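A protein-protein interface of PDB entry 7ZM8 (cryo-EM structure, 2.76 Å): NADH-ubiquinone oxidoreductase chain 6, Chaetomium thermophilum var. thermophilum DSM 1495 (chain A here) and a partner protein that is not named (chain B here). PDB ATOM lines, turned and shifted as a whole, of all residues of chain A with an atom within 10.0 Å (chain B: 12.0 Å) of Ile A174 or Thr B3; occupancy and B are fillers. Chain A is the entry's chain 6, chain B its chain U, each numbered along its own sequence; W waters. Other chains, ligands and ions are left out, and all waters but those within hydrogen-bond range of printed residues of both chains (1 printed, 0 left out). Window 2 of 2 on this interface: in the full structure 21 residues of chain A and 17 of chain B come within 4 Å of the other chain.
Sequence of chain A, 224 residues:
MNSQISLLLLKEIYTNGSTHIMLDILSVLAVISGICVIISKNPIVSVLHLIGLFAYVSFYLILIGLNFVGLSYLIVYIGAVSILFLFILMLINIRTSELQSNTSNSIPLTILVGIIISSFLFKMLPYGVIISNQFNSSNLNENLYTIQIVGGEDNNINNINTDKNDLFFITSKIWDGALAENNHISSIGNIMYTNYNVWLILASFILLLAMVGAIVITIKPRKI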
ATOM      1  N   PHE A 169       8.131  -7.930 -22.653  1.00  0.00           N
ATOM      2  CA  PHE A 169       6.802  -7.509 -23.161  1.00  0.00           C
ATOM      3  C   PHE A 169       5.745  -7.895 -22.130  1.00  0.00           C
ATOM      4  O   PHE A 169       5.565  -9.087 -21.881  1.00  0.00           O
ATOM      5  CB  PHE A 169       6.504  -8.192 -24.495  1.00  0.00           C
ATOM      6  CG  PHE A 169       7.192  -7.587 -25.688  1.00  0.00           C
ATOM      7  CD1 PHE A 169       6.612  -6.535 -26.376  1.00  0.00           C
ATOM      8  CD2 PHE A 169       8.412  -8.073 -26.123  1.00  0.00           C
ATOM      9  CE1 PHE A 169       7.241  -5.981 -27.477  1.00  0.00           C
ATOM     10  CE2 PHE A 169       9.040  -7.517 -27.223  1.00  0.00           C
ATOM     11  CZ  PHE A 169       8.453  -6.473 -27.897  1.00  0.00           C
ATOM     12  N   ILE A 170       5.075  -6.902 -21.553  1.00  0.00           N
ATOM     13  CA  ILE A 170       4.041  -7.160 -20.509  1.00  0.00           C
ATOM     14  C   ILE A 170       2.664  -7.315 -21.159  1.00  0.00           C
ATOM     15  O   ILE A 170       2.391  -6.613 -22.136  1.00  0.00           O
ATOM     16  CB  ILE A 170       4.071  -6.093 -19.391  1.00  0.00           C
ATOM     17  CG1 ILE A 170       3.305  -6.535 -18.142  1.00  0.00           C
ATOM     18  CG2 ILE A 170       3.620  -4.729 -19.886  1.00  0.00           C
ATOM     19  CD1 ILE A 170       4.120  -7.377 -17.198  1.00  0.00           C
ATOM     20  N   THR A 171       1.859  -8.253 -20.662  1.00  0.00           N
ATOM     21  CA  THR A 171       0.472  -8.404 -21.158  1.00  0.00           C
ATOM     22  C   THR A 171      -0.483  -8.590 -19.983  1.00  0.00           C
ATOM     23  O   THR A 171      -0.073  -9.195 -18.992  1.00  0.00           O
ATOM     24  CB  THR A 171       0.320  -9.590 -22.123  1.00  0.00           C
ATOM     25  OG1 THR A 171       0.982 -10.733 -21.583  1.00  0.00           O
ATOM     26  CG2 THR A 171       0.828  -9.306 -23.519  1.00  0.00           C
ATOM     27  N   SER A 172      -1.712  -8.094 -20.098  1.00  0.00           N
ATOM     28  CA  SER A 172      -2.730  -8.297 -19.078  1.00  0.00           C
ATOM     29  C   SER A 172      -4.020  -8.756 -19.739  1.00  0.00           C
ATOM     30  O   SER A 172      -4.055  -8.960 -20.956  1.00  0.00           O
ATOM     31  CB  SER A 172      -2.958  -7.016 -18.279  1.00  0.00           C
ATOM     32  OG  SER A 172      -4.213  -7.040 -17.629  1.00  0.00           O
ATOM     33  N   LYS A 173      -5.085  -8.943 -18.950  1.00  0.00           N
ATOM     34  CA  LYS A 173      -6.374  -9.491 -19.446  1.00  0.00           C
ATOM     35  C   LYS A 173      -7.421  -8.391 -19.661  1.00  0.00           C
ATOM     36  O   LYS A 173      -7.318  -7.363 -18.989  1.00  0.00           O
ATOM     37  CB  LYS A 173      -6.835 -10.528 -18.418  1.00  0.00           C
ATOM     38  CG  LYS A 173      -7.463 -10.006 -17.139  1.00  0.00           C
ATOM     39  CD  LYS A 173      -8.075 -11.110 -16.307  1.00  0.00           C
ATOM     40  CE  LYS A 173      -7.232 -12.367 -16.267  1.00  0.00           C
ATOM     41  NZ  LYS A 173      -7.650 -13.295 -15.189  1.00  0.00           N
ATOM     42  N   ILE A 174      -8.388  -8.594 -20.561  1.00  0.00           N
ATOM     43  CA  ILE A 174      -9.513  -7.630 -20.788  1.00  0.00           C
ATOM     44  C   ILE A 174     -10.814  -8.428 -20.784  1.00  0.00           C
ATOM     45  O   ILE A 174     -10.761  -9.609 -21.098  1.00  0.00           O
ATOM     46  CB  ILE A 174      -9.358  -6.829 -22.103  1.00  0.00           C
ATOM     47  CG1 ILE A 174     -10.324  -5.649 -22.192  1.00  0.00           C
ATOM     48  CG2 ILE A 174      -9.463  -7.728 -23.324  1.00  0.00           C
ATOM     49  CD1 ILE A 174     -10.106  -4.804 -23.419  1.00  0.00           C
ATOM     50  N   TRP A 175     -11.946  -7.792 -20.486  1.00  0.00           N
ATOM     51  CA  TRP A 175     -13.218  -8.549 -20.371  1.00  0.00           C
ATOM     52  C   TRP A 175     -14.208  -8.138 -21.459  1.00  0.00           C
ATOM     53  O   TRP A 175     -14.816  -9.030 -22.067  1.00  0.00           O
ATOM     54  CB  TRP A 175     -13.791  -8.397 -18.962  1.00  0.00           C
ATOM     55  CG  TRP A 175     -12.938  -9.081 -17.940  1.00  0.00           C
ATOM     56  CD1 TRP A 175     -12.042  -8.502 -17.091  1.00  0.00           C
ATOM     57  CD2 TRP A 175     -12.869 -10.495 -17.691  1.00  0.00           C
ATOM     58  NE1 TRP A 175     -11.441  -9.453 -16.315  1.00  0.00           N
ATOM     59  CE2 TRP A 175     -11.925 -10.685 -16.661  1.00  0.00           C
ATOM     60  CE3 TRP A 175     -13.517 -11.613 -18.228  1.00  0.00           C
ATOM     61  CZ2 TRP A 175     -11.619 -11.947 -16.157  1.00  0.00           C
ATOM     62  CZ3 TRP A 175     -13.214 -12.858 -17.730  1.00  0.00           C
ATOM     63  CH2 TRP A 175     -12.281 -13.019 -16.707  1.00  0.00           C
ATOM     64  N   ASP A 176     -14.368  -6.838 -21.681  1.00  0.00           N
ATOM     65  CA  ASP A 176     -15.292  -6.336 -22.731  1.00  0.00           C
ATOM     66  C   ASP A 176     -14.811  -6.787 -24.118  1.00  0.00           C
ATOM     67  O   ASP A 176     -15.674  -7.093 -24.959  1.00  0.00           O
ATOM     68  CB  ASP A 176     -15.627  -4.848 -22.552  1.00  0.00           C
ATOM     69  CG  ASP A 176     -14.453  -3.945 -22.217  1.00  0.00           C
ATOM     70  OD1 ASP A 176     -13.303  -4.382 -22.392  1.00  0.00           O
ATOM     71  OD2 ASP A 176     -14.704  -2.805 -21.788  1.00  0.00           O
ATOM     72  N   GLY A 177     -13.499  -6.810 -24.348  1.00  0.00           N
ATOM     73  CA  GLY A 177     -12.938  -7.250 -25.639  1.00  0.00           C
ATOM     74  C   GLY A 177     -12.758  -8.756 -25.736  1.00  0.00           C
ATOM     75  O   GLY A 177     -12.207  -9.207 -26.751  1.00  0.00           O
ATOM     76  N   ALA A 178     -13.185  -9.513 -24.724  1.00  0.00           N
ATOM     77  CA  ALA A 178     -13.130 -10.991 -24.758  1.00  0.00           C
ATOM     78  C   ALA A 178     -14.522 -11.606 -24.835  1.00  0.00           C
ATOM     79  O   ALA A 178     -14.575 -12.834 -24.746  1.00  0.00           O
ATOM     80  CB  ALA A 178     -12.430 -11.476 -23.517  1.00  0.00           C
ATOM     81  N   LEU A 179     -15.598 -10.828 -24.970  1.00  0.00           N
ATOM     82  CA  LEU A 179     -16.979 -11.397 -24.897  1.00  0.00           C
ATOM     83  C   LEU A 179     -17.161 -12.559 -25.870  1.00  0.00           C
ATOM     84  O   LEU A 179     -17.608 -13.611 -25.435  1.00  0.00           O
ATOM     85  CB  LEU A 179     -18.016 -10.306 -25.175  1.00  0.00           C
ATOM     86  CG  LEU A 179     -19.470 -10.758 -25.302  1.00  0.00           C
ATOM     87  CD1 LEU A 179     -20.032 -11.182 -23.957  1.00  0.00           C
ATOM     88  CD2 LEU A 179     -20.327  -9.654 -25.898  1.00  0.00           C
ATOM     89  N   ALA A 180     -16.807 -12.363 -27.132  1.00  0.00           N
ATOM     90  CA  ALA A 180     -16.990 -13.388 -28.168  1.00  0.00           C
ATOM     91  C   ALA A 180     -15.738 -13.420 -29.025  1.00  0.00           C
ATOM     92  O   ALA A 180     -15.840 -13.103 -30.199  1.00  0.00           O
ATOM     93  CB  ALA A 180     -18.174 -12.987 -28.988  1.00  0.00           C
ATOM     94  N   GLU A 181     -14.609 -13.828 -28.475  1.00  0.00           N
ATOM     95  CA  GLU A 181     -13.349 -13.769 -29.250  1.00  0.00           C
ATOM     96  C   GLU A 181     -13.425 -14.712 -30.449  1.00  0.00           C
ATOM     97  O   GLU A 181     -13.966 -15.825 -30.317  1.00  0.00           O
ATOM     98  CB  GLU A 181     -12.120 -13.975 -28.362  1.00  0.00           C
ATOM     99  CG  GLU A 181     -10.839 -14.318 -29.097  1.00  0.00           C
ATOM    100  CD  GLU A 181     -10.500 -15.800 -29.119  1.00  0.00           C
ATOM    101  OE1 GLU A 181     -11.176 -16.567 -28.408  1.00  0.00           O
ATOM    102  OE2 GLU A 181      -9.569 -16.186 -29.851  1.00  0.00           O
ATOM    103  N   MET B   1      -2.022  -3.779 -18.973  1.00  0.00           N
ATOM    104  CA  MET B   1      -0.916  -4.097 -19.908  1.00  0.00           C
ATOM    105  C   MET B   1      -1.509  -4.528 -21.229  1.00  0.00           C
ATOM    106  O   MET B   1      -2.732  -4.636 -21.283  1.00  0.00           O
ATOM    107  CB  MET B   1      -0.003  -5.190 -19.367  1.00  0.00           C
ATOM    108  N   ALA B   2      -0.681  -4.848 -22.211  1.00  0.00           N
ATOM    109  CA  ALA B   2      -1.202  -5.107 -23.567  1.00  0.00           C
ATOM    110  C   ALA B   2      -2.232  -6.223 -23.583  1.00  0.00           C
ATOM    111  O   ALA B   2      -2.063  -7.191 -22.859  1.00  0.00           O
ATOM    112  CB  ALA B   2      -0.072  -5.368 -24.503  1.00  0.00           C
ATOM    113  N   THR B   3      -3.269  -6.074 -24.410  1.00  0.00           N
ATOM    114  CA  THR B   3      -4.380  -7.057 -24.469  1.00  0.00           C
ATOM    115  C   THR B   3      -4.052  -8.194 -25.433  1.00  0.00           C
ATOM    116  O   THR B   3      -4.899  -9.077 -25.606  1.00  0.00           O
ATOM    117  CB  THR B   3      -5.676  -6.373 -24.908  1.00  0.00           C
ATOM    118  OG1 THR B   3      -5.447  -5.774 -26.182  1.00  0.00           O
ATOM    119  CG2 THR B   3      -6.153  -5.318 -23.939  1.00  0.00           C
ATOM    120  N   ARG B   4      -2.880  -8.170 -26.045  1.00  0.00           N
ATOM    121  CA  ARG B   4      -2.451  -9.274 -26.931  1.00  0.00           C
ATOM    122  C   ARG B   4      -2.369 -10.562 -26.130  1.00  0.00           C
ATOM    123  O   ARG B   4      -1.901 -10.508 -25.003  1.00  0.00           O
ATOM    124  CB  ARG B   4      -1.044  -8.974 -27.446  1.00  0.00           C
ATOM    125  CG  ARG B   4      -0.407 -10.114 -28.221  1.00  0.00           C
ATOM    126  CD  ARG B   4       1.025  -9.832 -28.612  1.00  0.00           C
ATOM    127  NE  ARG B   4       1.814  -9.216 -27.560  1.00  0.00           N
ATOM    128  CZ  ARG B   4       2.572  -9.873 -26.695  1.00  0.00           C
ATOM    129  NH1 ARG B   4       3.258  -9.207 -25.783  1.00  0.00           N
ATOM    130  NH2 ARG B   4       2.644 -11.190 -26.743  1.00  0.00           N
ATOM    131  N   LYS B   5      -2.844 -11.674 -26.690  1.00  0.00           N
ATOM    132  CA  LYS B   5      -2.686 -12.982 -26.026  1.00  0.00           C
ATOM    133  C   LYS B   5      -1.188 -13.307 -26.033  1.00  0.00           C
ATOM    134  O   LYS B   5      -0.555 -13.127 -27.086  1.00  0.00           O
ATOM    135  CB  LYS B   5      -3.479 -13.992 -26.841  1.00  0.00           C
ATOM    136  CG  LYS B   5      -4.977 -13.731 -26.931  1.00  0.00           C
ATOM    137  CD  LYS B   5      -5.627 -14.448 -28.094  1.00  0.00           C
ATOM    138  CE  LYS B   5      -7.069 -14.821 -27.826  1.00  0.00           C
ATOM    139  NZ  LYS B   5      -7.169 -15.918 -26.836  1.00  0.00           N
ATOM    140  N   PRO B   6      -0.582 -13.786 -24.927  1.00  0.00           N
ATOM    141  CA  PRO B   6       0.828 -14.134 -24.952  1.00  0.00           C
ATOM    142  C   PRO B   6       1.182 -15.502 -25.569  1.00  0.00           C
ATOM    143  O   PRO B   6       0.432 -16.430 -25.390  1.00  0.00           O
ATOM    144  CB  PRO B   6       1.165 -14.002 -23.469  1.00  0.00           C
ATOM    145  CG  PRO B   6      -0.080 -14.452 -22.752  1.00  0.00           C
ATOM    146  CD  PRO B   6      -1.215 -13.967 -23.623  1.00  0.00           C
ATOM    147  N   ALA B   7       2.333 -15.601 -26.246  1.00  0.00           N
ATOM    148  CA  ALA B   7       2.727 -16.852 -26.869  1.00  0.00           C
ATOM    149  C   ALA B   7       3.883 -17.552 -26.176  1.00  0.00           C
ATOM    150  O   ALA B   7       3.929 -18.785 -26.195  1.00  0.00           O
ATOM    151  CB  ALA B   7       3.106 -16.620 -28.342  1.00  0.00           C
ATOM    152  N   ASN B   9       5.044 -16.763 -22.762  1.00  0.00           N
ATOM    153  CA  ASN B   9       5.063 -16.222 -21.378  1.00  0.00           C
ATOM    154  C   ASN B   9       5.599 -17.290 -20.423  1.00  0.00           C
ATOM    155  O   ASN B   9       5.018 -18.364 -20.386  1.00  0.00           O
ATOM    156  CB  ASN B   9       3.665 -15.779 -20.939  1.00  0.00           C
ATOM    157  CG  ASN B   9       2.559 -16.742 -21.325  1.00  0.00           C
ATOM    158  OD1 ASN B   9       2.486 -17.207 -22.459  1.00  0.00           O
ATOM    159  ND2 ASN B   9       1.667 -17.028 -20.393  1.00  0.00           N
ATOM    160  N   TYR B  54     -21.897   2.458 -15.947  1.00  0.00           N
ATOM    161  CA  TYR B  54     -20.425   2.347 -15.973  1.00  0.00           C
ATOM    162  C   TYR B  54     -19.916   2.287 -17.406  1.00  0.00           C
ATOM    163  O   TYR B  54     -18.947   2.978 -17.725  1.00  0.00           O
ATOM    164  CB  TYR B  54     -20.014   1.158 -15.114  1.00  0.00           C
ATOM    165  CG  TYR B  54     -18.579   0.734 -15.217  1.00  0.00           C
ATOM    166  CD1 TYR B  54     -17.575   1.463 -14.609  1.00  0.00           C
ATOM    167  CD2 TYR B  54     -18.238  -0.412 -15.908  1.00  0.00           C
ATOM    168  CE1 TYR B  54     -16.256   1.063 -14.693  1.00  0.00           C
ATOM    169  CE2 TYR B  54     -16.925  -0.827 -16.005  1.00  0.00           C
ATOM    170  CZ  TYR B  54     -15.939  -0.084 -15.394  1.00  0.00           C
ATOM    171  OH  TYR B  54     -14.654  -0.504 -15.489  1.00  0.00           O
ATOM    172  N   MET B  55     -20.552   1.473 -18.229  1.00  0.00           N
ATOM    173  CA  MET B  55     -20.136   1.330 -19.644  1.00  0.00           C
ATOM    174  C   MET B  55     -20.382   2.632 -20.393  1.00  0.00           C
ATOM    175  O   MET B  55     -19.505   3.030 -21.151  1.00  0.00           O
ATOM    176  CB  MET B  55     -20.890   0.155 -20.268  1.00  0.00           C
ATOM    177  CG  MET B  55     -20.610  -1.148 -19.549  1.00  0.00           C
ATOM    178  SD  MET B  55     -18.872  -1.634 -19.595  1.00  0.00           S
ATOM    179  CE  MET B  55     -18.697  -2.059 -21.325  1.00  0.00           C
ATOM    180  N   LYS B  58     -17.561   5.265 -19.339  1.00  0.00           N
ATOM    181  CA  LYS B  58     -16.238   5.019 -19.969  1.00  0.00           C
ATOM    182  C   LYS B  58     -16.302   5.419 -21.431  1.00  0.00           C
ATOM    183  O   LYS B  58     -15.268   5.797 -21.969  1.00  0.00           O
ATOM    184  CB  LYS B  58     -15.918   3.527 -19.905  1.00  0.00           C
ATOM    185  CG  LYS B  58     -15.653   2.962 -18.519  1.00  0.00           C
ATOM    186  CD  LYS B  58     -14.735   1.770 -18.557  1.00  0.00           C
ATOM    187  CE  LYS B  58     -13.412   2.079 -19.222  1.00  0.00           C
ATOM    188  NZ  LYS B  58     -12.378   1.071 -18.888  1.00  0.00           N
ATOM    189  N   ASN B  59     -17.460   5.233 -22.052  1.00  0.00           N
ATOM    190  CA  ASN B  59     -17.673   5.586 -23.470  1.00  0.00           C
ATOM    191  C   ASN B  59     -17.605   7.098 -23.602  1.00  0.00           C
ATOM    192  O   ASN B  59     -17.103   7.575 -24.627  1.00  0.00           O
ATOM    193  CB  ASN B  59     -19.002   5.030 -23.965  1.00  0.00           C
ATOM    194  CG  ASN B  59     -18.864   3.911 -24.974  1.00  0.00           C
ATOM    195  OD1 ASN B  59     -17.768   3.439 -25.244  1.00  0.00           O
ATOM    196  ND2 ASN B  59     -19.979   3.487 -25.542  1.00  0.00           N
ATOM    197  N   GLY B  63     -10.266   6.856 -24.032  1.00  0.00           N
ATOM    198  CA  GLY B  63      -8.825   6.829 -23.710  1.00  0.00           C
ATOM    199  C   GLY B  63      -8.554   7.232 -22.280  1.00  0.00           C
ATOM    200  O   GLY B  63      -7.401   7.181 -21.876  1.00  0.00           O
ATOM    201  N   GLY B  65     -10.972   6.388 -19.572  1.00  0.00           N
ATOM    202  CA  GLY B  65     -12.089   5.828 -18.794  1.00  0.00           C
ATOM    203  C   GLY B  65     -11.685   4.930 -17.660  1.00  0.00           C
ATOM    204  O   GLY B  65     -12.527   4.743 -16.781  1.00  0.00           O
ATOM    205  N   GLU B  66     -10.479   4.363 -17.664  1.00  0.00           N
ATOM    206  CA  GLU B  66     -10.065   3.575 -16.476  1.00  0.00           C
ATOM    207  C   GLU B  66     -10.041   4.539 -15.298  1.00  0.00           C
ATOM    208  O   GLU B  66     -10.610   4.204 -14.270  1.00  0.00           O
ATOM    209  CB  GLU B  66      -8.707   2.957 -16.795  1.00  0.00           C
ATOM    210  CG  GLU B  66      -8.754   1.905 -17.890  1.00  0.00           C
ATOM    211  CD  GLU B  66      -8.907   2.386 -19.327  1.00  0.00           C
ATOM    212  OE1 GLU B  66      -8.558   3.551 -19.613  1.00  0.00           O
ATOM    213  OE2 GLU B  66      -9.385   1.591 -20.160  1.00  0.00           O
HETATM  214  O   HOH W   1       3.059  -6.344 -25.079  1.00  0.00           O
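Printed residues of chain B within 4 Å of Phe A169: Arg B4.
Of the printed residues of chain B, Ile A174 touches Thr B3.
No residue of chain B comes within 4 Å of Trp A175.
No residue of chain B comes within 4 Å of Asp A176.
No residue of chain B comes within 4 Å of Gly A177.
No residue of chain B comes within 4 Å of Ala A178.
Leu A179 touches none of the printed residues of chain B.
Printed residues of chain B within 4 Å of Glu A181: Lys B5.
Printed residues of chain A within 4 Å of Met B1: Ile A170 (3.7 Å), Thr A171 (3.5 Å) and Ser A172 (3.4 Å).
Of the printed residues of chain A, Thr B3 touches Ile A174 (3.99 Å).
Gly B63 touches none of the printed residues of chain A.
The nearest printed residue of chain B that does not touch Ile A174 is Ala B2 (6.9 Å).
Among the printed residues, pairs that only touch across the chains: Phe A169 with Arg B4 (3.6 Å), Ile A170 with Met B1 (3.7 Å), Ile A170 with Ala B2 (3.5 Å), Thr A171 with Met B1 (3.5 Å), Thr A171 with Ala B2 (3.3 Å), Thr A171 with Arg B4 (3.3 Å), Thr A171 with Pro B6 (3.8 Å), Ser A172 with Met B1 (3.4 Å) and Ile A174 with Thr B3 (3.99 Å).
Hydrophobic or aromatic side chains of chain A that line the printed part of chain B: Phe A169, Ile A170 and Ile A174.
Of the 15 printed residues of chain B, 6 touch a printed residue of chain A.
Printed residues of chain B that touch a printed residue of chain A: Met B1, Ala B2, Thr B3, Arg B4, Lys B5 and Pro B6.
Hydrophobic or aromatic side chains of chain B within 4 Å of the printed part of chain A: Met B1, Ala B2 and Pro B6.
Among the printed residues, 11 pairs touch across the chains.
Among the printed residues, Asp or Glu carboxylates within 4 Å of a Lys or Arg side-chain nitrogen of the other chain: Glu A181 with Lys B5 (3.9 Å).
The backbone carbonyl oxygen (O) of Ala B2 sits at hydrogen-bond distance from the backbone NH (N) of Ser A172 (2.9 Å).
OE2 of Glu A181 is in salt-bridge range of NZ of Lys B5 (3.9 Å).
Water W1 lies within hydrogen-bond range of the guanidinium group of Arg B4 and the backbone carbonyl oxygen of Ile A170.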
